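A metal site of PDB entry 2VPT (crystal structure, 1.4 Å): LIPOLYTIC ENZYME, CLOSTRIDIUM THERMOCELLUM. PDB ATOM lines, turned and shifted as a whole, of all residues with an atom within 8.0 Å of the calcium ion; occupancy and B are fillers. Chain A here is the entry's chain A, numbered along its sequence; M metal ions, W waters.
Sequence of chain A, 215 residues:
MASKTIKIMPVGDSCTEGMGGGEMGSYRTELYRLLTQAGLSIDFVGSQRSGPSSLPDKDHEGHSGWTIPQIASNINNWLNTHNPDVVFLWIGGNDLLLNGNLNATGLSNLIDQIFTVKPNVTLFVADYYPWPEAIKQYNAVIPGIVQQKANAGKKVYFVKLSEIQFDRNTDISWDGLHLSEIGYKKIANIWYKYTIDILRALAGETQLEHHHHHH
The backbone carbonyl oxygen of Asp 43 lies within hydrogen-bond range of the backbone NH of Ile 8.
NH1 of Arg 49 lies within salt-bridge range of OD1 of Asp 59.
Within 4 Å of the calcium ion: Asp 43, Phe 44, Asp 57 and Asp 59.
Along chain A the residues within 4 Å of the calcium ion span positions 43 to 59.
The nearest printed residue that does not touch the calcium ion is Val 45 (4.5 Å).
The calcium ion is bound by O of Phe 44 (2.3 Å), water W2 (2.3 Å), OD1 of Asp 43 (2.3 Å), OD2 of Asp 59 (2.4 Å), water W1 (2.4 Å), OD1 of Asp 57 (2.5 Å) and OD2 of Asp 57 (2.5 Å).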
ATOM      1  N   LYS A   7       7.195 -15.746  11.695  1.00  0.00           N
ATOM      2  CA  LYS A   7       6.019 -15.277  12.440  1.00  0.00           C
ATOM      3  C   LYS A   7       6.422 -14.075  13.286  1.00  0.00           C
ATOM      4  O   LYS A   7       7.320 -14.161  14.131  1.00  0.00           O
ATOM      5  CB  LYS A   7       5.456 -16.367  13.357  1.00  0.00           C
ATOM      6  CG  LYS A   7       4.800 -17.524  12.594  1.00  0.00           C
ATOM      7  CD  LYS A   7       4.241 -18.574  13.539  1.00  0.00           C
ATOM      8  CE  LYS A   7       3.412 -19.607  12.793  1.00  0.00           C
ATOM      9  NZ  LYS A   7       2.735 -20.574  13.704  1.00  0.00           N
ATOM     10  N   ILE A   8       5.758 -12.947  13.029  1.00  0.00           N
ATOM     11  CA  ILE A   8       6.037 -11.697  13.702  1.00  0.00           C
ATOM     12  C   ILE A   8       4.779 -11.248  14.432  1.00  0.00           C
ATOM     13  O   ILE A   8       3.720 -11.162  13.823  1.00  0.00           O
ATOM     14  CB  ILE A   8       6.460 -10.587  12.721  1.00  0.00           C
ATOM     15  CG1 ILE A   8       7.696 -10.999  11.909  1.00  0.00           C
ATOM     16  CG2 ILE A   8       6.703  -9.299  13.515  1.00  0.00           C
ATOM     17  CD1 ILE A   8       8.141 -10.001  10.842  1.00  0.00           C
ATOM     18  N   TYR A  32       4.323  -4.845   5.621  1.00  0.00           N
ATOM     19  CA  TYR A  32       4.083  -6.150   5.001  1.00  0.00           C
ATOM     20  C   TYR A  32       4.507  -6.108   3.529  1.00  0.00           C
ATOM     21  O   TYR A  32       5.123  -7.077   3.046  1.00  0.00           O
ATOM     22  CB  TYR A  32       2.616  -6.551   5.131  1.00  0.00           C
ATOM     23  CG  TYR A  32       2.358  -7.986   4.744  1.00  0.00           C
ATOM     24  CD1 TYR A  32       2.616  -9.018   5.620  1.00  0.00           C
ATOM     25  CD2 TYR A  32       1.918  -8.310   3.464  1.00  0.00           C
ATOM     26  CE1 TYR A  32       2.421 -10.330   5.278  1.00  0.00           C
ATOM     27  CE2 TYR A  32       1.722  -9.624   3.108  1.00  0.00           C
ATOM     28  CZ  TYR A  32       1.961 -10.632   4.005  1.00  0.00           C
ATOM     29  OH  TYR A  32       1.769 -11.956   3.678  1.00  0.00           O
ATOM     30  N   ILE A  42       6.353 -13.589   5.383  1.00  0.00           N
ATOM     31  CA  ILE A  42       5.963 -13.039   6.688  1.00  0.00           C
ATOM     32  C   ILE A  42       4.559 -13.494   7.056  1.00  0.00           C
ATOM     33  O   ILE A  42       3.634 -13.399   6.234  1.00  0.00           O
ATOM     34  CB  ILE A  42       5.993 -11.490   6.654  1.00  0.00           C
ATOM     35  CG1 ILE A  42       7.399 -10.996   6.301  1.00  0.00           C
ATOM     36  CG2 ILE A  42       5.526 -10.895   7.990  1.00  0.00           C
ATOM     37  CD1 ILE A  42       8.517 -11.468   7.229  1.00  0.00           C
ATOM     38  N   ASP A  43       4.405 -13.961   8.286  1.00  0.00           N
ATOM     39  CA  ASP A  43       3.117 -14.235   8.886  1.00  0.00           C
ATOM     40  C   ASP A  43       3.002 -13.326  10.116  1.00  0.00           C
ATOM     41  O   ASP A  43       3.643 -13.562  11.139  1.00  0.00           O
ATOM     42  CB  ASP A  43       3.020 -15.705   9.277  1.00  0.00           C
ATOM     43  CG  ASP A  43       1.665 -16.114   9.798  1.00  0.00           C
ATOM     44  OD1 ASP A  43       0.703 -15.301   9.763  1.00  0.00           O
ATOM     45  OD2 ASP A  43       1.560 -17.280  10.264  1.00  0.00           O
ATOM     46  N   PHE A  44       2.207 -12.260  10.007  1.00  0.00           N
ATOM     47  CA  PHE A  44       1.866 -11.484  11.184  1.00  0.00           C
ATOM     48  C   PHE A  44       0.925 -12.329  12.024  1.00  0.00           C
ATOM     49  O   PHE A  44      -0.026 -12.904  11.510  1.00  0.00           O
ATOM     50  CB  PHE A  44       1.192 -10.158  10.812  1.00  0.00           C
ATOM     51  CG  PHE A  44       2.129  -9.052  10.380  1.00  0.00           C
ATOM     52  CD1 PHE A  44       3.329  -8.808  11.050  1.00  0.00           C
ATOM     53  CD2 PHE A  44       1.766  -8.182   9.361  1.00  0.00           C
ATOM     54  CE1 PHE A  44       4.141  -7.767  10.651  1.00  0.00           C
ATOM     55  CE2 PHE A  44       2.581  -7.123   8.987  1.00  0.00           C
ATOM     56  CZ  PHE A  44       3.768  -6.919   9.629  1.00  0.00           C
ATOM     57  N   VAL A  45       1.195 -12.417  13.323  1.00  0.00           N
ATOM     58  CA  VAL A  45       0.380 -13.199  14.216  1.00  0.00           C
ATOM     59  C   VAL A  45      -0.153 -12.387  15.397  1.00  0.00           C
ATOM     60  O   VAL A  45       0.445 -11.409  15.835  1.00  0.00           O
ATOM     61  CB  VAL A  45       1.150 -14.465  14.719  1.00  0.00           C
ATOM     62  CG1 VAL A  45       1.564 -15.360  13.543  1.00  0.00           C
ATOM     63  CG2 VAL A  45       2.378 -14.087  15.559  1.00  0.00           C
ATOM     64  N   GLY A  46      -1.276 -12.837  15.917  1.00  0.00           N
ATOM     65  CA  GLY A  46      -1.979 -12.168  17.004  1.00  0.00           C
ATOM     66  C   GLY A  46      -3.462 -12.393  16.878  1.00  0.00           C
ATOM     67  O   GLY A  46      -3.942 -12.808  15.813  1.00  0.00           O
ATOM     68  N   GLN A  48      -5.978 -10.088  17.414  1.00  0.00           N
ATOM     69  CA  GLN A  48      -6.705  -8.953  16.832  1.00  0.00           C
ATOM     70  C   GLN A  48      -6.664  -9.091  15.320  1.00  0.00           C
ATOM     71  O   GLN A  48      -5.770  -9.741  14.782  1.00  0.00           O
ATOM     72  CB  GLN A  48      -6.035  -7.634  17.186  1.00  0.00           C
ATOM     73  CG  GLN A  48      -5.879  -7.361  18.682  1.00  0.00           C
ATOM     74  CD  GLN A  48      -7.123  -6.821  19.302  1.00  0.00           C
ATOM     75  OE1 GLN A  48      -8.101  -7.544  19.485  1.00  0.00           O
ATOM     76  NE2 GLN A  48      -7.101  -5.534  19.627  1.00  0.00           N
ATOM     77  N   ARG A  49      -7.625  -8.491  14.626  1.00  0.00           N
ATOM     78  CA  ARG A  49      -7.571  -8.478  13.161  1.00  0.00           C
ATOM     79  C   ARG A  49      -8.211  -7.193  12.654  1.00  0.00           C
ATOM     80  O   ARG A  49      -9.387  -6.913  12.895  1.00  0.00           O
ATOM     81  CB  ARG A  49      -8.205  -9.740  12.556  1.00  0.00           C
ATOM     82  CG  ARG A  49      -8.107  -9.851  11.018  1.00  0.00           C
ATOM     83  CD  ARG A  49      -7.805 -11.276  10.443  1.00  0.00           C
ATOM     84  NE  ARG A  49      -8.261 -12.422  11.239  1.00  0.00           N
ATOM     85  CZ  ARG A  49      -7.777 -13.671  11.170  1.00  0.00           C
ATOM     86  NH1 ARG A  49      -6.775 -14.000  10.353  1.00  0.00           N
ATOM     87  NH2 ARG A  49      -8.291 -14.616  11.935  1.00  0.00           N
ATOM     88  N   PRO A  56      -2.847  -8.124   3.144  1.00  0.00           N
ATOM     89  CA  PRO A  56      -3.278  -9.531   3.142  1.00  0.00           C
ATOM     90  C   PRO A  56      -3.359 -10.182   4.514  1.00  0.00           C
ATOM     91  O   PRO A  56      -4.177 -11.056   4.737  1.00  0.00           O
ATOM     92  CB  PRO A  56      -2.240 -10.217   2.231  1.00  0.00           C
ATOM     93  CG  PRO A  56      -1.674  -9.104   1.419  1.00  0.00           C
ATOM     94  CD  PRO A  56      -1.599  -7.957   2.371  1.00  0.00           C
ATOM     95  N   ASP A  57      -2.496  -9.752   5.421  1.00  0.00           N
ATOM     96  CA  ASP A  57      -2.355 -10.376   6.718  1.00  0.00           C
ATOM     97  C   ASP A  57      -2.603  -9.316   7.804  1.00  0.00           C
ATOM     98  O   ASP A  57      -1.739  -8.478   8.085  1.00  0.00           O
ATOM     99  CB  ASP A  57      -0.969 -11.009   6.873  1.00  0.00           C
ATOM    100  CG  ASP A  57      -0.883 -11.913   8.083  1.00  0.00           C
ATOM    101  OD1 ASP A  57      -1.706 -11.738   9.010  1.00  0.00           O
ATOM    102  OD2 ASP A  57       0.010 -12.807   8.117  1.00  0.00           O
ATOM    103  N   LYS A  58      -3.800  -9.369   8.365  1.00  0.00           N
ATOM    104  CA  LYS A  58      -4.320  -8.311   9.226  1.00  0.00           C
ATOM    105  C   LYS A  58      -4.220  -8.664  10.717  1.00  0.00           C
ATOM    106  O   LYS A  58      -4.732  -7.928  11.575  1.00  0.00           O
ATOM    107  CB  LYS A  58      -5.765  -8.004   8.862  1.00  0.00           C
ATOM    108  CG  LYS A  58      -5.962  -7.511   7.426  1.00  0.00           C
ATOM    109  CD  LYS A  58      -7.448  -7.494   7.003  1.00  0.00           C
ATOM    110  CE  LYS A  58      -7.679  -7.287   5.486  1.00  0.00           C
ATOM    111  NZ  LYS A  58      -7.261  -8.449   4.676  1.00  0.00           N
ATOM    112  N   ASP A  59      -3.538  -9.767  11.040  1.00  0.00           N
ATOM    113  CA  ASP A  59      -3.439 -10.213  12.437  1.00  0.00           C
ATOM    114  C   ASP A  59      -2.439  -9.373  13.228  1.00  0.00           C
ATOM    115  O   ASP A  59      -1.396  -8.985  12.699  1.00  0.00           O
ATOM    116  CB  ASP A  59      -3.003 -11.667  12.499  1.00  0.00           C
ATOM    117  CG  ASP A  59      -3.887 -12.566  11.660  1.00  0.00           C
ATOM    118  OD1 ASP A  59      -5.128 -12.462  11.755  1.00  0.00           O
ATOM    119  OD2 ASP A  59      -3.323 -13.366  10.883  1.00  0.00           O
ATOM    120  N   HIS A  60      -2.747  -9.119  14.489  1.00  0.00           N
ATOM    121  CA  HIS A  60      -1.829  -8.339  15.335  1.00  0.00           C
ATOM    122  C   HIS A  60      -2.223  -8.430  16.804  1.00  0.00           C
ATOM    123  O   HIS A  60      -3.243  -9.023  17.153  1.00  0.00           O
ATOM    124  CB  HIS A  60      -1.779  -6.878  14.894  1.00  0.00           C
ATOM    125  CG  HIS A  60      -3.070  -6.141  15.028  1.00  0.00           C
ATOM    126  ND1 HIS A  60      -3.467  -5.532  16.202  1.00  0.00           N
ATOM    127  CD2 HIS A  60      -4.067  -5.915  14.137  1.00  0.00           C
ATOM    128  CE1 HIS A  60      -4.643  -4.949  16.028  1.00  0.00           C
ATOM    129  NE2 HIS A  60      -5.030  -5.174  14.778  1.00  0.00           N
ATOM    130  N   HIS A  82       0.492 -17.900  20.039  1.00  0.00           N
ATOM    131  CA  HIS A  82       0.914 -17.586  18.669  1.00  0.00           C
ATOM    132  C   HIS A  82       2.354 -17.973  18.347  1.00  0.00           C
ATOM    133  O   HIS A  82       2.719 -18.047  17.173  1.00  0.00           O
ATOM    134  CB  HIS A  82       0.681 -16.107  18.383  1.00  0.00           C
ATOM    135  CG  HIS A  82      -0.758 -15.717  18.481  1.00  0.00           C
ATOM    136  ND1 HIS A  82      -1.701 -16.142  17.576  1.00  0.00           N
ATOM    137  CD2 HIS A  82      -1.421 -14.998  19.412  1.00  0.00           C
ATOM    138  CE1 HIS A  82      -2.887 -15.675  17.933  1.00  0.00           C
ATOM    139  NE2 HIS A  82      -2.749 -14.987  19.050  1.00  0.00           N
HETATM  140 CA    CA M   1      -1.242 -13.993   9.927  1.00  0.00          CA
HETATM  141  O   HOH W   1      -1.897 -15.745  11.419  1.00  0.00           O
HETATM  142  O   HOH W   2      -2.444 -14.935   8.175  1.00  0.00           O
